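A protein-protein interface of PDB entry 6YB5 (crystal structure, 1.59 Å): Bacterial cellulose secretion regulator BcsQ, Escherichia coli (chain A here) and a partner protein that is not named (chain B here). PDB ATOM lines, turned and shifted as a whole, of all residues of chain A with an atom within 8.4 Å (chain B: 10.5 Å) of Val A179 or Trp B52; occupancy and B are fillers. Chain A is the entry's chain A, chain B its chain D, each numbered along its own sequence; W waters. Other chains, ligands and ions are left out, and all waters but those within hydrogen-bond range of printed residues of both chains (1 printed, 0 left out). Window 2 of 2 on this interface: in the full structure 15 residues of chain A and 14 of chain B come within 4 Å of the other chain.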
ATOM      1  N   VAL A 149      20.457  17.227  29.882  1.00  0.00           N
ATOM      2  CA  VAL A 149      19.204  16.754  29.296  1.00  0.00           C
ATOM      3  C   VAL A 149      19.043  15.270  29.604  1.00  0.00           C
ATOM      4  O   VAL A 149      19.547  14.411  28.869  1.00  0.00           O
ATOM      5  CB  VAL A 149      19.133  17.014  27.777  1.00  0.00           C
ATOM      6  CG1 VAL A 149      17.784  16.527  27.218  1.00  0.00           C
ATOM      7  CG2 VAL A 149      19.301  18.521  27.481  1.00  0.00           C
ATOM      8  N   ASP A 150      18.365  14.961  30.707  1.00  0.00           N
ATOM      9  CA  ASP A 150      18.147  13.577  31.091  1.00  0.00           C
ATOM     10  C   ASP A 150      16.887  13.505  31.941  1.00  0.00           C
ATOM     11  O   ASP A 150      16.306  14.525  32.312  1.00  0.00           O
ATOM     12  CB  ASP A 150      19.386  12.974  31.795  1.00  0.00           C
ATOM     13  CG  ASP A 150      19.790  13.698  33.079  1.00  0.00           C
ATOM     14  OD1 ASP A 150      18.916  14.090  33.878  1.00  0.00           O
ATOM     15  OD2 ASP A 150      21.021  13.805  33.327  1.00  0.00           O
ATOM     16  N   ALA A 151      16.450  12.278  32.233  1.00  0.00           N
ATOM     17  CA  ALA A 151      15.155  12.133  32.883  1.00  0.00           C
ATOM     18  C   ALA A 151      15.159  12.695  34.298  1.00  0.00           C
ATOM     19  O   ALA A 151      14.122  13.187  34.760  1.00  0.00           O
ATOM     20  CB  ALA A 151      14.721  10.668  32.885  1.00  0.00           C
ATOM     21  N   HIS A 154      14.718  16.380  34.061  1.00  0.00           N
ATOM     22  CA  HIS A 154      13.347  16.626  33.606  1.00  0.00           C
ATOM     23  C   HIS A 154      12.367  16.585  34.772  1.00  0.00           C
ATOM     24  O   HIS A 154      11.544  17.493  34.949  1.00  0.00           O
ATOM     25  CB  HIS A 154      12.958  15.597  32.546  1.00  0.00           C
ATOM     26  CG  HIS A 154      11.584  15.799  31.989  1.00  0.00           C
ATOM     27  ND1 HIS A 154      11.290  16.799  31.087  1.00  0.00           N
ATOM     28  CD2 HIS A 154      10.427  15.126  32.200  1.00  0.00           C
ATOM     29  CE1 HIS A 154      10.011  16.727  30.756  1.00  0.00           C
ATOM     30  NE2 HIS A 154       9.462  15.728  31.425  1.00  0.00           N
ATOM     31  N   PHE A 173      25.635  18.024  26.593  1.00  0.00           N
ATOM     32  CA  PHE A 173      24.744  17.538  25.543  1.00  0.00           C
ATOM     33  C   PHE A 173      25.466  16.515  24.668  1.00  0.00           C
ATOM     34  O   PHE A 173      26.559  16.784  24.159  1.00  0.00           O
ATOM     35  CB  PHE A 173      24.260  18.730  24.704  1.00  0.00           C
ATOM     36  CG  PHE A 173      22.993  18.474  23.920  1.00  0.00           C
ATOM     37  CD1 PHE A 173      21.773  18.370  24.576  1.00  0.00           C
ATOM     38  CD2 PHE A 173      23.020  18.400  22.539  1.00  0.00           C
ATOM     39  CE1 PHE A 173      20.588  18.172  23.865  1.00  0.00           C
ATOM     40  CE2 PHE A 173      21.840  18.201  21.818  1.00  0.00           C
ATOM     41  CZ  PHE A 173      20.621  18.085  22.497  1.00  0.00           C
ATOM     42  N   ARG A 174      24.850  15.343  24.487  1.00  0.00           N
ATOM     43  CA  ARG A 174      25.487  14.233  23.786  1.00  0.00           C
ATOM     44  C   ARG A 174      25.144  14.190  22.296  1.00  0.00           C
ATOM     45  O   ARG A 174      24.141  14.739  21.833  1.00  0.00           O
ATOM     46  CB  ARG A 174      25.067  12.896  24.401  1.00  0.00           C
ATOM     47  CG  ARG A 174      25.317  12.731  25.873  1.00  0.00           C
ATOM     48  CD  ARG A 174      24.803  11.357  26.317  1.00  0.00           C
ATOM     49  NE  ARG A 174      25.421  10.262  25.562  1.00  0.00           N
ATOM     50  CZ  ARG A 174      26.649   9.814  25.800  1.00  0.00           C
ATOM     51  NH1 ARG A 174      27.377  10.367  26.765  1.00  0.00           N
ATOM     52  NH2 ARG A 174      27.154   8.817  25.078  1.00  0.00           N
ATOM     53  N   GLY A 176      23.907  11.595  19.519  1.00  0.00           N
ATOM     54  CA  GLY A 176      23.359  10.272  19.260  1.00  0.00           C
ATOM     55  C   GLY A 176      22.694   9.597  20.442  1.00  0.00           C
ATOM     56  O   GLY A 176      23.027   8.461  20.791  1.00  0.00           O
ATOM     57  N   SER A 177      21.748  10.284  21.075  1.00  0.00           N
ATOM     58  CA  SER A 177      20.936   9.693  22.128  1.00  0.00           C
ATOM     59  C   SER A 177      19.479  10.018  21.842  1.00  0.00           C
ATOM     60  O   SER A 177      19.091  11.190  21.872  1.00  0.00           O
ATOM     61  CB  SER A 177      21.333  10.234  23.500  1.00  0.00           C
ATOM     62  OG  SER A 177      20.351   9.897  24.465  1.00  0.00           O
ATOM     63  N   GLN A 178      18.673   8.987  21.572  1.00  0.00           N
ATOM     64  CA  GLN A 178      17.277   9.237  21.227  1.00  0.00           C
ATOM     65  C   GLN A 178      16.501   9.797  22.412  1.00  0.00           C
ATOM     66  O   GLN A 178      15.718  10.743  22.253  1.00  0.00           O
ATOM     67  CB  GLN A 178      16.606   7.960  20.719  1.00  0.00           C
ATOM     68  CG  GLN A 178      15.162   8.210  20.292  1.00  0.00           C
ATOM     69  CD  GLN A 178      15.067   9.124  19.074  1.00  0.00           C
ATOM     70  OE1 GLN A 178      14.429  10.185  19.118  1.00  0.00           O
ATOM     71  NE2 GLN A 178      15.702   8.717  17.977  1.00  0.00           N
ATOM     72  N   VAL A 179      16.685   9.229  23.606  1.00  0.00           N
ATOM     73  CA  VAL A 179      15.922   9.746  24.740  1.00  0.00           C
ATOM     74  C   VAL A 179      16.320  11.188  25.025  1.00  0.00           C
ATOM     75  O   VAL A 179      15.471  12.014  25.367  1.00  0.00           O
ATOM     76  CB  VAL A 179      16.063   8.844  25.984  1.00  0.00           C
ATOM     77  CG1 VAL A 179      17.486   8.836  26.532  1.00  0.00           C
ATOM     78  CG2 VAL A 179      15.070   9.285  27.068  1.00  0.00           C
ATOM     79  N   GLN A 180      17.603  11.528  24.854  1.00  0.00           N
ATOM     80  CA  GLN A 180      18.009  12.925  25.019  1.00  0.00           C
ATOM     81  C   GLN A 180      17.308  13.819  24.005  1.00  0.00           C
ATOM     82  O   GLN A 180      16.786  14.884  24.356  1.00  0.00           O
ATOM     83  CB  GLN A 180      19.521  13.076  24.880  1.00  0.00           C
ATOM     84  CG  GLN A 180      19.966  14.537  24.970  1.00  0.00           C
ATOM     85  CD  GLN A 180      21.412  14.714  24.576  1.00  0.00           C
ATOM     86  OE1 GLN A 180      22.298  14.728  25.435  1.00  0.00           O
ATOM     87  NE2 GLN A 180      21.660  14.863  23.274  1.00  0.00           N
ATOM     88  N   ASP A 181      17.294  13.410  22.732  1.00  0.00           N
ATOM     89  CA  ASP A 181      16.651  14.245  21.723  1.00  0.00           C
ATOM     90  C   ASP A 181      15.163  14.402  22.012  1.00  0.00           C
ATOM     91  O   ASP A 181      14.589  15.476  21.791  1.00  0.00           O
ATOM     92  CB  ASP A 181      16.868  13.648  20.338  1.00  0.00           C
ATOM     93  CG  ASP A 181      16.564  14.638  19.229  1.00  0.00           C
ATOM     94  OD1 ASP A 181      17.364  15.583  19.038  1.00  0.00           O
ATOM     95  OD2 ASP A 181      15.526  14.480  18.554  1.00  0.00           O
ATOM     96  N   ASP A 182      14.522  13.349  22.523  1.00  0.00           N
ATOM     97  CA  ASP A 182      13.092  13.441  22.808  1.00  0.00           C
ATOM     98  C   ASP A 182      12.818  14.426  23.936  1.00  0.00           C
ATOM     99  O   ASP A 182      11.898  15.255  23.844  1.00  0.00           O
ATOM    100  CB  ASP A 182      12.534  12.056  23.155  1.00  0.00           C
ATOM    101  CG  ASP A 182      12.503  11.120  21.952  1.00  0.00           C
ATOM    102  OD1 ASP A 182      12.532  11.617  20.802  1.00  0.00           O
ATOM    103  OD2 ASP A 182      12.442   9.888  22.159  1.00  0.00           O
ATOM    104  N   ILE A 183      13.602  14.346  25.016  1.00  0.00           N
ATOM    105  CA  ILE A 183      13.450  15.302  26.111  1.00  0.00           C
ATOM    106  C   ILE A 183      13.718  16.717  25.621  1.00  0.00           C
ATOM    107  O   ILE A 183      12.974  17.660  25.942  1.00  0.00           O
ATOM    108  CB  ILE A 183      14.377  14.933  27.287  1.00  0.00           C
ATOM    109  CG1 ILE A 183      13.960  13.598  27.902  1.00  0.00           C
ATOM    110  CG2 ILE A 183      14.325  16.027  28.348  1.00  0.00           C
ATOM    111  CD1 ILE A 183      14.971  13.032  28.898  1.00  0.00           C
ATOM    112  N   TYR A 184      14.785  16.889  24.838  1.00  0.00           N
ATOM    113  CA  TYR A 184      15.173  18.216  24.360  1.00  0.00           C
ATOM    114  C   TYR A 184      14.092  18.815  23.474  1.00  0.00           C
ATOM    115  O   TYR A 184      13.723  19.981  23.637  1.00  0.00           O
ATOM    116  CB  TYR A 184      16.495  18.122  23.605  1.00  0.00           C
ATOM    117  CG  TYR A 184      16.985  19.424  23.035  1.00  0.00           C
ATOM    118  CD1 TYR A 184      17.297  20.480  23.871  1.00  0.00           C
ATOM    119  CD2 TYR A 184      17.167  19.582  21.665  1.00  0.00           C
ATOM    120  CE1 TYR A 184      17.771  21.678  23.362  1.00  0.00           C
ATOM    121  CE2 TYR A 184      17.643  20.772  21.149  1.00  0.00           C
ATOM    122  CZ  TYR A 184      17.947  21.808  22.009  1.00  0.00           C
ATOM    123  OH  TYR A 184      18.414  23.009  21.509  1.00  0.00           O
ATOM    124  N   GLN A 185      13.570  18.033  22.525  1.00  0.00           N
ATOM    125  CA  GLN A 185      12.518  18.561  21.654  1.00  0.00           C
ATOM    126  C   GLN A 185      11.288  18.962  22.466  1.00  0.00           C
ATOM    127  O   GLN A 185      10.647  19.986  22.183  1.00  0.00           O
ATOM    128  CB  GLN A 185      12.156  17.532  20.580  1.00  0.00           C
ATOM    129  CG  GLN A 185      13.277  17.286  19.567  1.00  0.00           C
ATOM    130  CD  GLN A 185      13.688  18.549  18.820  1.00  0.00           C
ATOM    131  OE1 GLN A 185      12.842  19.340  18.399  1.00  0.00           O
ATOM    132  NE2 GLN A 185      14.998  18.749  18.665  1.00  0.00           N
ATOM    133  N   LEU A 186      10.951  18.175  23.487  1.00  0.00           N
ATOM    134  CA  LEU A 186       9.843  18.530  24.367  1.00  0.00           C
ATOM    135  C   LEU A 186      10.134  19.819  25.126  1.00  0.00           C
ATOM    136  O   LEU A 186       9.253  20.678  25.260  1.00  0.00           O
ATOM    137  CB  LEU A 186       9.566  17.377  25.339  1.00  0.00           C
ATOM    138  CG  LEU A 186       8.426  17.582  26.338  1.00  0.00           C
ATOM    139  CD1 LEU A 186       7.110  17.889  25.620  1.00  0.00           C
ATOM    140  CD2 LEU A 186       8.293  16.349  27.216  1.00  0.00           C
ATOM    141  N   TYR B  36       2.527  23.147  28.705  1.00  0.00           N
ATOM    142  CA  TYR B  36       2.223  22.033  27.815  1.00  0.00           C
ATOM    143  C   TYR B  36       1.015  22.289  26.915  1.00  0.00           C
ATOM    144  O   TYR B  36       0.484  21.346  26.323  1.00  0.00           O
ATOM    145  CB  TYR B  36       2.007  20.756  28.627  1.00  0.00           C
ATOM    146  CG  TYR B  36       3.273  20.199  29.232  1.00  0.00           C
ATOM    147  CD1 TYR B  36       4.289  19.697  28.421  1.00  0.00           C
ATOM    148  CD2 TYR B  36       3.456  20.161  30.611  1.00  0.00           C
ATOM    149  CE1 TYR B  36       5.448  19.174  28.967  1.00  0.00           C
ATOM    150  CE2 TYR B  36       4.618  19.641  31.169  1.00  0.00           C
ATOM    151  CZ  TYR B  36       5.608  19.152  30.343  1.00  0.00           C
ATOM    152  OH  TYR B  36       6.751  18.639  30.900  1.00  0.00           O
ATOM    153  N   GLN B  44       5.697  15.996  15.709  1.00  0.00           N
ATOM    154  CA  GLN B  44       7.052  15.536  15.995  1.00  0.00           C
ATOM    155  C   GLN B  44       7.181  15.041  17.430  1.00  0.00           C
ATOM    156  O   GLN B  44       8.004  14.162  17.714  1.00  0.00           O
ATOM    157  CB  GLN B  44       8.055  16.659  15.729  1.00  0.00           C
ATOM    158  CG  GLN B  44       9.513  16.220  15.725  1.00  0.00           C
ATOM    159  CD  GLN B  44       9.929  15.580  14.414  1.00  0.00           C
ATOM    160  OE1 GLN B  44      10.597  16.207  13.591  1.00  0.00           O
ATOM    161  NE2 GLN B  44       9.538  14.326  14.213  1.00  0.00           N
ATOM    162  N   LEU B  45       6.376  15.585  18.345  1.00  0.00           N
ATOM    163  CA  LEU B  45       6.422  15.186  19.744  1.00  0.00           C
ATOM    164  C   LEU B  45       5.567  13.968  20.050  1.00  0.00           C
ATOM    165  O   LEU B  45       5.742  13.361  21.113  1.00  0.00           O
ATOM    166  CB  LEU B  45       5.970  16.345  20.639  1.00  0.00           C
ATOM    167  CG  LEU B  45       6.925  17.532  20.684  1.00  0.00           C
ATOM    168  CD1 LEU B  45       6.456  18.540  21.711  1.00  0.00           C
ATOM    169  CD2 LEU B  45       8.336  17.061  21.005  1.00  0.00           C
ATOM    170  N   ALA B  46       4.642  13.610  19.155  1.00  0.00           N
ATOM    171  CA  ALA B  46       3.717  12.513  19.425  1.00  0.00           C
ATOM    172  C   ALA B  46       4.458  11.209  19.678  1.00  0.00           C
ATOM    173  O   ALA B  46       4.189  10.511  20.663  1.00  0.00           O
ATOM    174  CB  ALA B  46       2.739  12.357  18.259  1.00  0.00           C
ATOM    175  N   ALA B  47       5.394  10.857  18.792  1.00  0.00           N
ATOM    176  CA  ALA B  47       6.141   9.616  18.965  1.00  0.00           C
ATOM    177  C   ALA B  47       6.948   9.629  20.259  1.00  0.00           C
ATOM    178  O   ALA B  47       7.039   8.609  20.950  1.00  0.00           O
ATOM    179  CB  ALA B  47       7.055   9.380  17.762  1.00  0.00           C
ATOM    180  N   ALA B  48       7.525  10.780  20.611  1.00  0.00           N
ATOM    181  CA  ALA B  48       8.324  10.867  21.829  1.00  0.00           C
ATOM    182  C   ALA B  48       7.481  10.613  23.073  1.00  0.00           C
ATOM    183  O   ALA B  48       7.908   9.902  23.990  1.00  0.00           O
ATOM    184  CB  ALA B  48       9.000  12.233  21.909  1.00  0.00           C
ATOM    185  N   LEU B  49       6.282  11.197  23.133  1.00  0.00           N
ATOM    186  CA  LEU B  49       5.427  10.985  24.295  1.00  0.00           C
ATOM    187  C   LEU B  49       4.936   9.546  24.374  1.00  0.00           C
ATOM    188  O   LEU B  49       4.757   9.013  25.476  1.00  0.00           O
ATOM    189  CB  LEU B  49       4.239  11.947  24.255  1.00  0.00           C
ATOM    190  CG  LEU B  49       4.592  13.428  24.376  1.00  0.00           C
ATOM    191  CD1 LEU B  49       3.339  14.274  24.147  1.00  0.00           C
ATOM    192  CD2 LEU B  49       5.227  13.725  25.728  1.00  0.00           C
ATOM    193  N   LYS B  50       4.709   8.905  23.229  1.00  0.00           N
ATOM    194  CA  LYS B  50       4.311   7.503  23.246  1.00  0.00           C
ATOM    195  C   LYS B  50       5.475   6.593  23.622  1.00  0.00           C
ATOM    196  O   LYS B  50       5.258   5.521  24.197  1.00  0.00           O
ATOM    197  CB  LYS B  50       3.737   7.108  21.885  1.00  0.00           C
ATOM    198  CG  LYS B  50       2.955   5.808  21.896  1.00  0.00           C
ATOM    199  CD  LYS B  50       2.151   5.638  20.611  1.00  0.00           C
ATOM    200  CE  LYS B  50       3.040   5.716  19.379  1.00  0.00           C
ATOM    201  NZ  LYS B  50       2.298   5.360  18.135  1.00  0.00           N
ATOM    202  N   ARG B  51       6.709   7.004  23.308  1.00  0.00           N
ATOM    203  CA  ARG B  51       7.877   6.185  23.624  1.00  0.00           C
ATOM    204  C   ARG B  51       8.146   6.143  25.126  1.00  0.00           C
ATOM    205  O   ARG B  51       8.570   5.111  25.658  1.00  0.00           O
ATOM    206  CB  ARG B  51       9.112   6.713  22.886  1.00  0.00           C
ATOM    207  CG  ARG B  51       9.230   6.297  21.419  1.00  0.00           C
ATOM    208  CD  ARG B  51      10.647   6.528  20.865  1.00  0.00           C
ATOM    209  NE  ARG B  51      10.920   7.927  20.538  1.00  0.00           N
ATOM    210  CZ  ARG B  51      10.599   8.495  19.379  1.00  0.00           C
ATOM    211  NH1 ARG B  51      10.876   9.775  19.157  1.00  0.00           N
ATOM    212  NH2 ARG B  51       9.995   7.782  18.437  1.00  0.00           N
ATOM    213  N   TRP B  52       7.916   7.250  25.823  1.00  0.00           N
ATOM    214  CA  TRP B  52       8.376   7.411  27.204  1.00  0.00           C
ATOM    215  C   TRP B  52       7.239   7.767  28.154  1.00  0.00           C
ATOM    216  O   TRP B  52       6.794   8.932  28.167  1.00  0.00           O
ATOM    217  CB  TRP B  52       9.469   8.479  27.270  1.00  0.00           C
ATOM    218  CG  TRP B  52      10.582   8.250  26.285  1.00  0.00           C
ATOM    219  CD1 TRP B  52      10.940   9.063  25.248  1.00  0.00           C
ATOM    220  CD2 TRP B  52      11.475   7.120  26.234  1.00  0.00           C
ATOM    221  NE1 TRP B  52      12.002   8.515  24.561  1.00  0.00           N
ATOM    222  CE2 TRP B  52      12.351   7.327  25.149  1.00  0.00           C
ATOM    223  CE3 TRP B  52      11.618   5.959  27.004  1.00  0.00           C
ATOM    224  CZ2 TRP B  52      13.352   6.415  24.808  1.00  0.00           C
ATOM    225  CZ3 TRP B  52      12.612   5.053  26.663  1.00  0.00           C
ATOM    226  CH2 TRP B  52      13.461   5.282  25.576  1.00  0.00           C
ATOM    227  N   PRO B  53       6.777   6.828  28.985  1.00  0.00           N
ATOM    228  CA  PRO B  53       5.682   7.144  29.919  1.00  0.00           C
ATOM    229  C   PRO B  53       6.009   8.270  30.879  1.00  0.00           C
ATOM    230  O   PRO B  53       5.095   9.000  31.292  1.00  0.00           O
ATOM    231  CB  PRO B  53       5.466   5.818  30.668  1.00  0.00           C
ATOM    232  CG  PRO B  53       6.035   4.780  29.771  1.00  0.00           C
ATOM    233  CD  PRO B  53       7.149   5.402  29.017  1.00  0.00           C
ATOM    234  N   LEU B  54       7.281   8.429  31.261  1.00  0.00           N
ATOM    235  CA  LEU B  54       7.647   9.532  32.144  1.00  0.00           C
ATOM    236  C   LEU B  54       7.306  10.873  31.507  1.00  0.00           C
ATOM    237  O   LEU B  54       6.768  11.767  32.175  1.00  0.00           O
ATOM    238  CB  LEU B  54       9.138   9.468  32.484  1.00  0.00           C
ATOM    239  CG  LEU B  54       9.583  10.510  33.514  1.00  0.00           C
ATOM    240  CD1 LEU B  54       9.077  10.143  34.920  1.00  0.00           C
ATOM    241  CD2 LEU B  54      11.104  10.714  33.497  1.00  0.00           C
ATOM    242  N   LEU B  55       7.611  11.036  30.214  1.00  0.00           N
ATOM    243  CA  LEU B  55       7.341  12.315  29.553  1.00  0.00           C
ATOM    244  C   LEU B  55       5.846  12.522  29.364  1.00  0.00           C
ATOM    245  O   LEU B  55       5.339  13.649  29.496  1.00  0.00           O
ATOM    246  CB  LEU B  55       8.054  12.370  28.200  1.00  0.00           C
ATOM    247  CG  LEU B  55       9.572  12.175  28.208  1.00  0.00           C
ATOM    248  CD1 LEU B  55      10.159  12.482  26.823  1.00  0.00           C
ATOM    249  CD2 LEU B  55      10.230  13.036  29.280  1.00  0.00           C
ATOM    250  N   ALA B  56       5.128  11.445  29.054  1.00  0.00           N
ATOM    251  CA  ALA B  56       3.695  11.556  28.821  1.00  0.00           C
ATOM    252  C   ALA B  56       2.962  11.989  30.084  1.00  0.00           C
ATOM    253  O   ALA B  56       1.997  12.762  30.018  1.00  0.00           O
ATOM    254  CB  ALA B  56       3.155  10.224  28.295  1.00  0.00           C
ATOM    255  N   GLU B  57       3.411  11.524  31.251  1.00  0.00           N
ATOM    256  CA  GLU B  57       2.614  11.780  32.448  1.00  0.00           C
ATOM    257  C   GLU B  57       2.690  13.238  32.884  1.00  0.00           C
ATOM    258  O   GLU B  57       1.736  13.747  33.483  1.00  0.00           O
ATOM    259  CB  GLU B  57       3.024  10.829  33.578  1.00  0.00           C
ATOM    260  CG  GLU B  57       4.093  11.318  34.517  1.00  0.00           C
ATOM    261  CD  GLU B  57       4.405  10.289  35.603  1.00  0.00           C
ATOM    262  OE1 GLU B  57       5.559   9.842  35.660  1.00  0.00           O
ATOM    263  OE2 GLU B  57       3.496   9.924  36.382  1.00  0.00           O
ATOM    264  N   PHE B  58       3.791  13.937  32.579  1.00  0.00           N
ATOM    265  CA  PHE B  58       3.842  15.367  32.868  1.00  0.00           C
ATOM    266  C   PHE B  58       3.059  16.181  31.850  1.00  0.00           C
ATOM    267  O   PHE B  58       2.497  17.225  32.198  1.00  0.00           O
ATOM    268  CB  PHE B  58       5.288  15.868  32.894  1.00  0.00           C
ATOM    269  CG  PHE B  58       6.088  15.353  34.050  1.00  0.00           C
ATOM    270  CD1 PHE B  58       5.891  15.868  35.325  1.00  0.00           C
ATOM    271  CD2 PHE B  58       7.041  14.374  33.866  1.00  0.00           C
ATOM    272  CE1 PHE B  58       6.643  15.394  36.403  1.00  0.00           C
ATOM    273  CE2 PHE B  58       7.793  13.891  34.938  1.00  0.00           C
ATOM    274  CZ  PHE B  58       7.589  14.407  36.206  1.00  0.00           C
ATOM    275  N   ALA B  59       3.032  15.728  30.598  1.00  0.00           N
ATOM    276  CA  ALA B  59       2.454  16.491  29.500  1.00  0.00           C
ATOM    277  C   ALA B  59       0.955  16.275  29.344  1.00  0.00           C
ATOM    278  O   ALA B  59       0.305  17.048  28.631  1.00  0.00           O
ATOM    279  CB  ALA B  59       3.165  16.137  28.184  1.00  0.00           C
ATOM    280  N   GLN B  60       0.393  15.263  30.003  1.00  0.00           N
ATOM    281  CA  GLN B  60      -1.029  14.971  29.882  1.00  0.00           C
ATOM    282  C   GLN B  60      -1.872  16.101  30.465  1.00  0.00           C
ATOM    283  O   GLN B  60      -1.444  16.831  31.365  1.00  0.00           O
ATOM    284  CB  GLN B  60      -1.363  13.661  30.592  1.00  0.00           C
ATOM    285  CG  GLN B  60      -1.240  13.747  32.108  1.00  0.00           C
ATOM    286  CD  GLN B  60      -1.341  12.392  32.785  1.00  0.00           C
ATOM    287  OE1 GLN B  60      -1.464  11.359  32.123  1.00  0.00           O
ATOM    288  NE2 GLN B  60      -1.286  12.390  34.112  1.00  0.00           N
HETATM  289  O   HOH W   1       7.055  15.749  30.110  1.00  0.00           O
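The side-chain carboxylate (OD2) of Asp A182 is in salt-bridge range of the guanidinium group (NE) of Arg B51 (3.0 Å).
NE1 of Trp B52 lies within hydrogen-bond range of OD2 of Asp A182, at 2.8 Å.
The side-chain amide oxygen of Gln A178 sits close to the side-chain carboxylate of Asp A182, at 2.9 Å.
Ala A151 touches Leu B54 (CB to CD2, 3.7 Å).
His A154 touches Tyr B36 (CE1 to OH, 3.8 Å).
NE2 of His A154 touches CD2 of Leu B55, 3.5 Å away.
NE2 of His A154 touches CD2 of Phe B58, 3.7 Å away.
Gln A178 touches Arg B51.
Val A179 touches Trp B52 (CB to CZ2, 3.8 Å).
CB of Ala B48 touches CG of Asp A182, 3.7 Å away.
Gln A185 touches Leu B45.
Leu A186 touches Tyr B36.
Leu A186 touches Leu B45.
Of chain B, only Trp B52 (3.8 Å) comes within 4 Å of Val A179.
Of chain A, only Val A179 (3.8 Å) and Asp A182 (2.8 Å) come within 4 Å of Trp B52.
No residue of chain B comes within 4 Å of Ser A177.
No residue of chain A comes within 4 Å of Pro B53.
Printed residues of chain A within 4 Å of Phe B58: His A154.
Printed residues of chain B within 4 Å of Leu A186: Tyr B36 (3.95 Å) and Leu B45 (3.8 Å).
Of the printed residues of chain A, Leu B55 touches His A154.
Of the printed residues of chain B, Gln A178 touches Arg B51.
Of the printed residues of chain A, Leu B54 touches Ala A151.
The nearest residue of chain B that does not touch Val A179 is Leu B55 (5.5 Å).
The nearest residue of chain A that does not touch Trp B52 is Gln A178 (4.9 Å).
The nearest printed residue of chain B that does not touch Gln A185 is Gln B44 (5.3 Å).
Of the 17 printed residues of chain A, 7 touch a printed residue of chain B.
Hydrophobic or aromatic side chains of chain A within 4 Å of the printed part of chain B: Ala A151, His A154, Val A179 and Leu A186.
Along chain A the printed residues that touch a printed residue of chain B span positions 151 to 186.
Hydrophobic or aromatic side chains of chain B that line the printed part of chain A: Tyr B36, Leu B45, Ala B48, Trp B52, Leu B54, Leu B55 and Phe B58.
Among the printed residues, Asp or Glu carboxylates within 4 Å of a Lys or Arg side-chain nitrogen of the other chain: Asp A182 with Arg B51 (3.0 Å).
Water W1 lies within hydrogen-bond range of a ring nitrogen (NE2) of His A154 (2.7 Å), the backbone carbonyl oxygen of Leu B55 (2.8 Å) and the side-chain hydroxyl of Tyr B36 (3.0 Å).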
